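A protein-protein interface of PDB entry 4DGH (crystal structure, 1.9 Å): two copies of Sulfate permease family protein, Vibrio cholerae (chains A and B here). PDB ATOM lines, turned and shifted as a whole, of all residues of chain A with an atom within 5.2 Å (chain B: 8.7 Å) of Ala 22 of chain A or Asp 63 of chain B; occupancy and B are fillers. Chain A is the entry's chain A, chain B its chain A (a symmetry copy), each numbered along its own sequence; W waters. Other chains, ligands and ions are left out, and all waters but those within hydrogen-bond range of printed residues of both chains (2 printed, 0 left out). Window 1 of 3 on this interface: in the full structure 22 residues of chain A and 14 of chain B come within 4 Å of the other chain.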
ATOM      1  N   LEU A  17     -19.859  -7.220  25.643  1.00  0.00           N
ATOM      2  CA  LEU A  17     -19.624  -5.908  26.197  1.00  0.00           C
ATOM      3  C   LEU A  17     -19.272  -6.146  27.670  1.00  0.00           C
ATOM      4  O   LEU A  17     -19.937  -6.958  28.371  1.00  0.00           O
ATOM      5  CB  LEU A  17     -20.946  -5.135  26.175  1.00  0.00           C
ATOM      6  CG  LEU A  17     -21.278  -4.193  25.016  1.00  0.00           C
ATOM      7  CD1 LEU A  17     -22.648  -3.590  25.404  1.00  0.00           C
ATOM      8  CD2 LEU A  17     -20.220  -3.092  24.891  1.00  0.00           C
ATOM      9  N   GLU A  20     -18.706  -3.145  32.891  1.00  0.00           N
ATOM     10  CA  GLU A  20     -18.496  -1.706  33.064  1.00  0.00           C
ATOM     11  C   GLU A  20     -19.014  -0.744  32.011  1.00  0.00           C
ATOM     12  O   GLU A  20     -19.016   0.450  32.295  1.00  0.00           O
ATOM     13  CB  GLU A  20     -17.027  -1.324  33.381  1.00  0.00           C
ATOM     14  CG  GLU A  20     -16.550  -2.055  34.592  1.00  0.00           C
ATOM     15  CD  GLU A  20     -15.923  -3.382  34.235  1.00  0.00           C
ATOM     16  OE1 GLU A  20     -16.207  -4.053  33.161  1.00  0.00           O
ATOM     17  OE2 GLU A  20     -15.016  -3.696  35.010  1.00  0.00           O
ATOM     18  N   LEU A  21     -19.471  -1.232  30.838  1.00  0.00           N
ATOM     19  CA  LEU A  21     -19.829  -0.298  29.762  1.00  0.00           C
ATOM     20  C   LEU A  21     -21.280  -0.564  29.340  1.00  0.00           C
ATOM     21  O   LEU A  21     -21.667  -1.736  29.113  1.00  0.00           O
ATOM     22  CB  LEU A  21     -18.892  -0.588  28.602  1.00  0.00           C
ATOM     23  CG  LEU A  21     -19.179   0.199  27.333  1.00  0.00           C
ATOM     24  CD1 LEU A  21     -18.950   1.670  27.644  1.00  0.00           C
ATOM     25  CD2 LEU A  21     -18.191  -0.262  26.308  1.00  0.00           C
ATOM     26  N   ALA A  22     -22.062   0.497  29.173  1.00  0.00           N
ATOM     27  CA  ALA A  22     -23.420   0.404  28.660  1.00  0.00           C
ATOM     28  C   ALA A  22     -23.498   1.314  27.416  1.00  0.00           C
ATOM     29  O   ALA A  22     -22.655   2.199  27.183  1.00  0.00           O
ATOM     30  CB  ALA A  22     -24.419   0.803  29.737  1.00  0.00           C
ATOM     31  N   VAL A  23     -24.505   1.071  26.596  1.00  0.00           N
ATOM     32  CA  VAL A  23     -24.613   1.802  25.341  1.00  0.00           C
ATOM     33  C   VAL A  23     -26.120   2.060  25.217  1.00  0.00           C
ATOM     34  O   VAL A  23     -26.950   1.120  25.388  1.00  0.00           O
ATOM     35  CB  VAL A  23     -24.136   0.950  24.166  1.00  0.00           C
ATOM     36  CG1 VAL A  23     -24.465   1.704  22.871  1.00  0.00           C
ATOM     37  CG2 VAL A  23     -22.643   0.684  24.267  1.00  0.00           C
ATOM     38  N   TYR A  24     -26.478   3.299  24.924  1.00  0.00           N
ATOM     39  CA  TYR A  24     -27.894   3.627  24.716  1.00  0.00           C
ATOM     40  C   TYR A  24     -28.032   4.527  23.519  1.00  0.00           C
ATOM     41  O   TYR A  24     -27.199   5.426  23.336  1.00  0.00           O
ATOM     42  CB  TYR A  24     -28.434   4.333  25.995  1.00  0.00           C
ATOM     43  CG  TYR A  24     -29.950   4.667  25.839  1.00  0.00           C
ATOM     44  CD1 TYR A  24     -30.938   3.630  25.840  1.00  0.00           C
ATOM     45  CD2 TYR A  24     -30.390   5.971  25.685  1.00  0.00           C
ATOM     46  CE1 TYR A  24     -32.301   3.918  25.669  1.00  0.00           C
ATOM     47  CE2 TYR A  24     -31.794   6.242  25.562  1.00  0.00           C
ATOM     48  CZ  TYR A  24     -32.686   5.231  25.478  1.00  0.00           C
ATOM     49  OH  TYR A  24     -34.062   5.534  25.308  1.00  0.00           O
ATOM     50  N   MET A  42     -31.932   3.622  35.029  1.00  0.00           N
ATOM     51  CA  MET A  42     -30.589   3.836  35.572  1.00  0.00           C
ATOM     52  C   MET A  42     -30.700   4.207  37.048  1.00  0.00           C
ATOM     53  O   MET A  42     -29.797   3.923  37.851  1.00  0.00           O
ATOM     54  CB  MET A  42     -29.909   4.959  34.764  1.00  0.00           C
ATOM     55  CG  MET A  42     -28.427   4.977  35.084  1.00  0.00           C
ATOM     56  SD  MET A  42     -27.609   3.392  34.194  1.00  0.00           S
ATOM     57  CE  MET A  42     -27.003   3.869  32.388  1.00  0.00           C
ATOM     58  N   PRO A  49     -23.236   1.024  35.307  1.00  0.00           N
ATOM     59  CA  PRO A  49     -22.003   0.872  34.560  1.00  0.00           C
ATOM     60  C   PRO A  49     -21.018   2.004  34.982  1.00  0.00           C
ATOM     61  O   PRO A  49     -21.464   2.997  35.512  1.00  0.00           O
ATOM     62  CB  PRO A  49     -22.470   1.078  33.073  1.00  0.00           C
ATOM     63  CG  PRO A  49     -23.718   1.920  33.163  1.00  0.00           C
ATOM     64  CD  PRO A  49     -24.325   1.676  34.557  1.00  0.00           C
ATOM     65  N   ILE A  51     -19.151   3.529  32.502  1.00  0.00           N
ATOM     66  CA  ILE A  51     -19.219   4.350  31.299  1.00  0.00           C
ATOM     67  C   ILE A  51     -20.504   4.064  30.534  1.00  0.00           C
ATOM     68  O   ILE A  51     -20.907   2.869  30.334  1.00  0.00           O
ATOM     69  CB  ILE A  51     -18.007   4.117  30.354  1.00  0.00           C
ATOM     70  CG1 ILE A  51     -16.669   4.378  31.151  1.00  0.00           C
ATOM     71  CG2 ILE A  51     -18.102   4.980  29.076  1.00  0.00           C
ATOM     72  CD1 ILE A  51     -15.390   4.124  30.348  1.00  0.00           C
ATOM     73  N   LEU A  52     -21.138   5.127  30.053  1.00  0.00           N
ATOM     74  CA  LEU A  52     -22.325   4.977  29.195  1.00  0.00           C
ATOM     75  C   LEU A  52     -22.112   5.764  27.894  1.00  0.00           C
ATOM     76  O   LEU A  52     -21.938   7.009  27.936  1.00  0.00           O
ATOM     77  CB  LEU A  52     -23.559   5.486  29.929  1.00  0.00           C
ATOM     78  CG  LEU A  52     -24.806   5.582  29.039  1.00  0.00           C
ATOM     79  CD1 LEU A  52     -25.259   4.234  28.487  1.00  0.00           C
ATOM     80  CD2 LEU A  52     -25.940   6.327  29.710  1.00  0.00           C
ATOM     81  N   ILE A  53     -22.143   5.064  26.754  1.00  0.00           N
ATOM     82  CA  ILE A  53     -22.102   5.735  25.462  1.00  0.00           C
ATOM     83  C   ILE A  53     -23.519   6.036  25.025  1.00  0.00           C
ATOM     84  O   ILE A  53     -24.356   5.137  24.885  1.00  0.00           O
ATOM     85  CB  ILE A  53     -21.318   4.949  24.397  1.00  0.00           C
ATOM     86  CG1 ILE A  53     -19.874   4.656  24.968  1.00  0.00           C
ATOM     87  CG2 ILE A  53     -21.316   5.645  23.047  1.00  0.00           C
ATOM     88  CD1 ILE A  53     -19.154   3.598  24.126  1.00  0.00           C
ATOM     89  N   PRO B  29     -32.457  -3.787  21.546  1.00  0.00           N
ATOM     90  CA  PRO B  29     -31.755  -3.770  22.794  1.00  0.00           C
ATOM     91  C   PRO B  29     -32.366  -2.917  23.898  1.00  0.00           C
ATOM     92  O   PRO B  29     -31.990  -3.082  25.034  1.00  0.00           O
ATOM     93  CB  PRO B  29     -30.376  -3.281  22.432  1.00  0.00           C
ATOM     94  CG  PRO B  29     -30.546  -2.565  21.135  1.00  0.00           C
ATOM     95  CD  PRO B  29     -31.865  -2.884  20.551  1.00  0.00           C
ATOM     96  N   PHE B  30     -33.225  -1.950  23.579  1.00  0.00           N
ATOM     97  CA  PHE B  30     -33.716  -1.029  24.627  1.00  0.00           C
ATOM     98  C   PHE B  30     -35.168  -1.410  24.894  1.00  0.00           C
ATOM     99  O   PHE B  30     -36.139  -0.678  24.547  1.00  0.00           O
ATOM    100  CB  PHE B  30     -33.531   0.452  24.132  1.00  0.00           C
ATOM    101  CG  PHE B  30     -32.165   0.707  23.511  1.00  0.00           C
ATOM    102  CD1 PHE B  30     -30.992   0.373  24.192  1.00  0.00           C
ATOM    103  CD2 PHE B  30     -32.052   1.268  22.226  1.00  0.00           C
ATOM    104  CE1 PHE B  30     -29.763   0.621  23.634  1.00  0.00           C
ATOM    105  CE2 PHE B  30     -30.809   1.476  21.665  1.00  0.00           C
ATOM    106  CZ  PHE B  30     -29.663   1.175  22.370  1.00  0.00           C
ATOM    107  N   PHE B  31     -35.311  -2.615  25.425  1.00  0.00           N
ATOM    108  CA  PHE B  31     -36.632  -3.219  25.569  1.00  0.00           C
ATOM    109  C   PHE B  31     -37.205  -2.765  26.909  1.00  0.00           C
ATOM    110  O   PHE B  31     -38.217  -3.237  27.288  1.00  0.00           O
ATOM    111  CB  PHE B  31     -36.530  -4.743  25.517  1.00  0.00           C
ATOM    112  CG  PHE B  31     -35.508  -5.300  26.513  1.00  0.00           C
ATOM    113  CD1 PHE B  31     -35.866  -5.490  27.855  1.00  0.00           C
ATOM    114  CD2 PHE B  31     -34.197  -5.580  26.108  1.00  0.00           C
ATOM    115  CE1 PHE B  31     -34.951  -5.987  28.782  1.00  0.00           C
ATOM    116  CE2 PHE B  31     -33.294  -6.062  27.044  1.00  0.00           C
ATOM    117  CZ  PHE B  31     -33.661  -6.235  28.377  1.00  0.00           C
ATOM    118  N   PHE B  32     -36.574  -1.788  27.584  1.00  0.00           N
ATOM    119  CA  PHE B  32     -36.973  -1.393  28.977  1.00  0.00           C
ATOM    120  C   PHE B  32     -38.435  -0.970  29.105  1.00  0.00           C
ATOM    121  O   PHE B  32     -39.117  -1.388  30.032  1.00  0.00           O
ATOM    122  CB  PHE B  32     -36.075  -0.250  29.578  1.00  0.00           C
ATOM    123  CG  PHE B  32     -34.607  -0.380  29.244  1.00  0.00           C
ATOM    124  CD1 PHE B  32     -33.814  -1.339  29.879  1.00  0.00           C
ATOM    125  CD2 PHE B  32     -34.034   0.413  28.251  1.00  0.00           C
ATOM    126  CE1 PHE B  32     -32.466  -1.507  29.535  1.00  0.00           C
ATOM    127  CE2 PHE B  32     -32.688   0.249  27.908  1.00  0.00           C
ATOM    128  CZ  PHE B  32     -31.907  -0.709  28.526  1.00  0.00           C
ATOM    129  N   VAL B  59     -32.727  -9.115  20.216  1.00  0.00           N
ATOM    130  CA  VAL B  59     -31.864  -8.347  21.105  1.00  0.00           C
ATOM    131  C   VAL B  59     -30.427  -8.523  20.664  1.00  0.00           C
ATOM    132  O   VAL B  59     -29.901  -9.623  20.747  1.00  0.00           O
ATOM    133  CB  VAL B  59     -32.000  -8.833  22.582  1.00  0.00           C
ATOM    134  CG1 VAL B  59     -31.016  -8.080  23.534  1.00  0.00           C
ATOM    135  CG2 VAL B  59     -33.443  -8.775  22.996  1.00  0.00           C
ATOM    136  N   PRO B  60     -29.788  -7.469  20.148  1.00  0.00           N
ATOM    137  CA  PRO B  60     -28.454  -7.677  19.607  1.00  0.00           C
ATOM    138  C   PRO B  60     -27.322  -7.686  20.658  1.00  0.00           C
ATOM    139  O   PRO B  60     -26.272  -8.256  20.416  1.00  0.00           O
ATOM    140  CB  PRO B  60     -28.281  -6.485  18.606  1.00  0.00           C
ATOM    141  CG  PRO B  60     -29.168  -5.428  19.164  1.00  0.00           C
ATOM    142  CD  PRO B  60     -30.327  -6.120  19.809  1.00  0.00           C
ATOM    143  N   PHE B  61     -27.532  -7.072  21.811  1.00  0.00           N
ATOM    144  CA  PHE B  61     -26.535  -7.060  22.847  1.00  0.00           C
ATOM    145  C   PHE B  61     -27.306  -6.693  24.121  1.00  0.00           C
ATOM    146  O   PHE B  61     -28.454  -6.245  24.041  1.00  0.00           O
ATOM    147  CB  PHE B  61     -25.380  -6.041  22.601  1.00  0.00           C
ATOM    148  CG  PHE B  61     -25.841  -4.609  22.645  1.00  0.00           C
ATOM    149  CD1 PHE B  61     -25.906  -3.902  23.879  1.00  0.00           C
ATOM    150  CD2 PHE B  61     -26.272  -3.968  21.469  1.00  0.00           C
ATOM    151  CE1 PHE B  61     -26.409  -2.591  23.906  1.00  0.00           C
ATOM    152  CE2 PHE B  61     -26.742  -2.648  21.494  1.00  0.00           C
ATOM    153  CZ  PHE B  61     -26.836  -1.981  22.740  1.00  0.00           C
ATOM    154  N   MET B  62     -26.676  -6.912  25.282  1.00  0.00           N
ATOM    155  CA  MET B  62     -27.294  -6.523  26.553  1.00  0.00           C
ATOM    156  C   MET B  62     -26.181  -6.028  27.434  1.00  0.00           C
ATOM    157  O   MET B  62     -25.082  -6.615  27.460  1.00  0.00           O
ATOM    158  CB  MET B  62     -27.860  -7.669  27.340  1.00  0.00           C
ATOM    159  CG  MET B  62     -29.002  -8.261  26.563  1.00  0.00           C
ATOM    160  SD  MET B  62     -30.039  -9.301  27.879  1.00  0.00           S
ATOM    161  CE  MET B  62     -30.848  -7.890  28.880  1.00  0.00           C
ATOM    162  N   ASP B  63     -26.394  -4.883  28.069  1.00  0.00           N
ATOM    163  CA  ASP B  63     -25.446  -4.413  29.052  1.00  0.00           C
ATOM    164  C   ASP B  63     -26.020  -4.703  30.429  1.00  0.00           C
ATOM    165  O   ASP B  63     -27.140  -5.270  30.553  1.00  0.00           O
ATOM    166  CB  ASP B  63     -25.084  -2.887  28.792  1.00  0.00           C
ATOM    167  CG  ASP B  63     -26.288  -1.962  28.787  1.00  0.00           C
ATOM    168  OD1 ASP B  63     -27.227  -2.196  29.581  1.00  0.00           O
ATOM    169  OD2 ASP B  63     -26.320  -0.970  27.967  1.00  0.00           O
ATOM    170  N   ILE B  64     -25.274  -4.275  31.464  1.00  0.00           N
ATOM    171  CA  ILE B  64     -25.710  -4.428  32.840  1.00  0.00           C
ATOM    172  C   ILE B  64     -27.124  -3.886  33.060  1.00  0.00           C
ATOM    173  O   ILE B  64     -27.863  -4.401  33.928  1.00  0.00           O
ATOM    174  CB  ILE B  64     -24.684  -3.822  33.853  1.00  0.00           C
ATOM    175  CG1 ILE B  64     -24.760  -4.562  35.213  1.00  0.00           C
ATOM    176  CG2 ILE B  64     -24.663  -2.266  33.793  1.00  0.00           C
ATOM    177  CD1 ILE B  64     -23.559  -4.242  36.130  1.00  0.00           C
ATOM    178  N   THR B  65     -27.502  -2.841  32.350  1.00  0.00           N
ATOM    179  CA  THR B  65     -28.806  -2.265  32.566  1.00  0.00           C
ATOM    180  C   THR B  65     -29.912  -3.192  32.021  1.00  0.00           C
ATOM    181  O   THR B  65     -30.974  -3.361  32.671  1.00  0.00           O
ATOM    182  CB  THR B  65     -28.989  -0.784  32.033  1.00  0.00           C
ATOM    183  OG1 THR B  65     -28.952  -0.804  30.628  1.00  0.00           O
ATOM    184  CG2 THR B  65     -27.842   0.143  32.459  1.00  0.00           C
ATOM    185  N   GLY B  66     -29.702  -3.799  30.852  1.00  0.00           N
ATOM    186  CA  GLY B  66     -30.750  -4.672  30.322  1.00  0.00           C
ATOM    187  C   GLY B  66     -30.698  -5.993  31.106  1.00  0.00           C
ATOM    188  O   GLY B  66     -31.697  -6.640  31.282  1.00  0.00           O
ATOM    189  N   ILE B  67     -29.527  -6.428  31.543  1.00  0.00           N
ATOM    190  CA  ILE B  67     -29.464  -7.655  32.371  1.00  0.00           C
ATOM    191  C   ILE B  67     -30.272  -7.522  33.641  1.00  0.00           C
ATOM    192  O   ILE B  67     -31.044  -8.416  33.993  1.00  0.00           O
ATOM    193  CB  ILE B  67     -28.005  -8.011  32.724  1.00  0.00           C
ATOM    194  CG1 ILE B  67     -27.417  -8.589  31.425  1.00  0.00           C
ATOM    195  CG2 ILE B  67     -27.969  -9.017  33.905  1.00  0.00           C
ATOM    196  CD1 ILE B  67     -27.852 -10.036  31.070  1.00  0.00           C
ATOM    197  N   GLN B  68     -30.128  -6.393  34.324  1.00  0.00           N
ATOM    198  CA  GLN B  68     -30.847  -6.227  35.583  1.00  0.00           C
ATOM    199  C   GLN B  68     -32.350  -6.040  35.330  1.00  0.00           C
ATOM    200  O   GLN B  68     -33.171  -6.487  36.117  1.00  0.00           O
ATOM    201  CB  GLN B  68     -30.284  -5.055  36.372  1.00  0.00           C
ATOM    202  CG  GLN B  68     -28.930  -5.416  36.983  1.00  0.00           C
ATOM    203  CD  GLN B  68     -28.200  -4.194  37.517  1.00  0.00           C
ATOM    204  OE1 GLN B  68     -27.580  -3.450  36.734  1.00  0.00           O
ATOM    205  NE2 GLN B  68     -28.224  -3.985  38.841  1.00  0.00           N
ATOM    206  N   THR B  69     -32.701  -5.424  34.214  1.00  0.00           N
ATOM    207  CA  THR B  69     -34.114  -5.333  33.817  1.00  0.00           C
ATOM    208  C   THR B  69     -34.706  -6.695  33.531  1.00  0.00           C
ATOM    209  O   THR B  69     -35.833  -7.001  33.965  1.00  0.00           O
ATOM    210  CB  THR B  69     -34.219  -4.364  32.623  1.00  0.00           C
ATOM    211  OG1 THR B  69     -33.703  -3.117  33.062  1.00  0.00           O
ATOM    212  CG2 THR B  69     -35.660  -4.105  32.192  1.00  0.00           C
ATOM    213  N   LEU B  70     -33.986  -7.513  32.742  1.00  0.00           N
ATOM    214  CA  LEU B  70     -34.471  -8.849  32.404  1.00  0.00           C
ATOM    215  C   LEU B  70     -34.584  -9.700  33.679  1.00  0.00           C
ATOM    216  O   LEU B  70     -35.529 -10.485  33.833  1.00  0.00           O
ATOM    217  CB  LEU B  70     -33.561  -9.528  31.378  1.00  0.00           C
ATOM    218  CG  LEU B  70     -33.822 -10.948  30.989  1.00  0.00           C
ATOM    219  CD1 LEU B  70     -35.215 -11.087  30.353  1.00  0.00           C
ATOM    220  CD2 LEU B  70     -32.861 -11.465  29.943  1.00  0.00           C
ATOM    221  N   VAL B  93     -25.179 -12.639  23.218  1.00  0.00           N
ATOM    222  CA  VAL B  93     -26.129 -12.550  24.312  1.00  0.00           C
ATOM    223  C   VAL B  93     -26.217 -13.903  25.058  1.00  0.00           C
ATOM    224  O   VAL B  93     -26.402 -13.888  26.284  1.00  0.00           O
ATOM    225  CB  VAL B  93     -27.507 -12.159  23.775  1.00  0.00           C
ATOM    226  CG1 VAL B  93     -28.564 -12.125  24.873  1.00  0.00           C
ATOM    227  CG2 VAL B  93     -27.378 -10.741  23.127  1.00  0.00           C
ATOM    228  N   LYS B  96     -23.561 -13.922  27.549  1.00  0.00           N
ATOM    229  CA  LYS B  96     -23.885 -12.945  28.600  1.00  0.00           C
ATOM    230  C   LYS B  96     -24.931 -13.498  29.565  1.00  0.00           C
ATOM    231  O   LYS B  96     -24.848 -13.278  30.760  1.00  0.00           O
ATOM    232  CB  LYS B  96     -24.465 -11.649  28.018  1.00  0.00           C
ATOM    233  CG  LYS B  96     -23.627 -10.454  28.068  1.00  0.00           C
ATOM    234  CD  LYS B  96     -23.877  -9.654  29.301  1.00  0.00           C
ATOM    235  CE  LYS B  96     -22.625  -8.852  29.401  1.00  0.00           C
ATOM    236  NZ  LYS B  96     -22.740  -7.680  28.528  1.00  0.00           N
ATOM    237  N   LEU B  97     -25.955 -14.188  29.040  1.00  0.00           N
ATOM    238  CA  LEU B  97     -27.012 -14.726  29.874  1.00  0.00           C
ATOM    239  C   LEU B  97     -26.417 -15.739  30.945  1.00  0.00           C
ATOM    240  O   LEU B  97     -26.891 -15.796  32.083  1.00  0.00           O
ATOM    241  CB  LEU B  97     -28.041 -15.459  29.016  1.00  0.00           C
ATOM    242  CG  LEU B  97     -28.883 -14.508  28.054  1.00  0.00           C
ATOM    243  CD1 LEU B  97     -29.968 -15.363  27.423  1.00  0.00           C
ATOM    244  CD2 LEU B  97     -29.491 -13.355  28.827  1.00  0.00           C
ATOM    245  N   ALA B 100     -24.107 -13.651  33.506  1.00  0.00           N
ATOM    246  CA  ALA B 100     -24.894 -12.809  34.372  1.00  0.00           C
ATOM    247  C   ALA B 100     -25.805 -13.519  35.336  1.00  0.00           C
ATOM    248  O   ALA B 100     -26.364 -12.861  36.225  1.00  0.00           O
ATOM    249  CB  ALA B 100     -25.704 -11.827  33.545  1.00  0.00           C
ATOM    250  N   ILE B 102     -28.560 -15.267  34.372  1.00  0.00           N
ATOM    251  CA  ILE B 102     -29.961 -15.391  33.876  1.00  0.00           C
ATOM    252  C   ILE B 102     -30.261 -16.875  33.650  1.00  0.00           C
ATOM    253  O   ILE B 102     -31.362 -17.367  33.943  1.00  0.00           O
ATOM    254  CB  ILE B 102     -30.235 -14.540  32.621  1.00  0.00           C
ATOM    255  CG1 ILE B 102     -30.020 -13.022  32.927  1.00  0.00           C
ATOM    256  CG2 ILE B 102     -31.650 -14.785  32.099  1.00  0.00           C
ATOM    257  CD1 ILE B 102     -30.884 -12.520  34.076  1.00  0.00           C
HETATM  258  O   HOH W   1     -28.730  -0.785  26.974  1.00  0.00           O
HETATM  259  O   HOH W   2     -22.865  -3.064  31.273  1.00  0.00           O
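The backbone NH (N) of Ala 22 of chain A is in hydrogen-bond range of the backbone carbonyl oxygen (O) of Ile 51 of chain A (2.9 Å). The backbone carbonyl oxygen (O) of Ala 22 of chain A lies within hydrogen-bond range of the backbone NH (N) of Ile 53 of chain A. The backbone NH of Tyr 24 of chain A lies within hydrogen-bond range of the backbone carbonyl oxygen of Ile 53 of chain A. The backbone carbonyl oxygen of Met 62 of chain B lies within hydrogen-bond range of the side-chain amino group of Lys 96 of chain B (2.8 Å). The side-chain carboxylate (OD1) of Asp 63 of chain B lies within hydrogen-bond range of the side-chain hydroxyl (OG1) of Thr 65 of chain B, at 2.5 Å. OD1 of Asp 63 of chain B is in hydrogen-bond range of N of Gly 66 of chain B.
NZ of Lys 96 of chain B is in hydrogen-bond range of O of Leu 17 of chain A (2.9 Å). OD2 of Asp 63 of chain B is in hydrogen-bond range of N of Val 23 of chain A (3.1 Å).
Phe 61 of chain B touches Leu 17 of chain A (CD1 to CD1, 3.6 Å). Leu 21 of chain A touches Asp 63 of chain B (O to CB, 3.6 Å). Asp 63 of chain B touches Ala 22 of chain A (OD2 to CB, 3.1 Å). Val 23 of chain A touches Phe 30 of chain B. Phe 30 of chain B touches Tyr 24 of chain A (CD1 to CD1, 3.7 Å). Met 42 of chain A touches Thr 65 of chain B (SD to CG2, 3.7 Å). Pro 49 of chain A touches Ile 64 of chain B (N to CG2, 3.9 Å).
Of the 11 printed residues of chain A, 7 touch a printed residue of chain B. Hydrophobic or aromatic side chains of chain A within 4 Å of the printed part of chain B: Leu 17, Ala 22, Tyr 24 and Met 42. Of the 21 printed residues of chain B, 6 touch a printed residue of chain A. Printed residues of chain B that touch a printed residue of chain A: Phe 30, Phe 61, Asp 63, Ile 64, Thr 65 and Lys 96.
Of chain B, only Asp 63 comes within 4 Å of Ala 22 of chain A. Asp 63 of chain B touches just these residues of chain A: Leu 21 (3.6 Å), Ala 22 (3.1 Å) and Val 23 (3.1 Å). Printed residues of chain B within 4 Å of Val 23 of chain A: Phe 30 (3.4 Å) and Asp 63 (3.1 Å). Of the printed residues of chain B, Tyr 24 of chain A touches Phe 30 (3.7 Å). Printed residues of chain A within 4 Å of Ile 64 of chain B: Pro 49. Ile 53 of chain A touches none of the printed residues of chain B. Pro 29 of chain B touches none of the printed residues of chain A. The nearest residue of chain A that does not touch Asp 63 of chain B is Leu 17 of chain A (4.2 Å).
No position is printed for both chains. Of the 9 pairs that touch across the chains among the printed residues, none has its exchanged pair printed and touching as well.
Water W1 lies within hydrogen-bond range of OD2 of Asp 63 of chain B (2.6 Å) and O of Val 23 of chain A (3.1 Å). Water W2 lies within hydrogen-bond range of N of Ile 64 of chain B (2.7 Å) and O of Leu 21 of chain A (2.8 Å).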
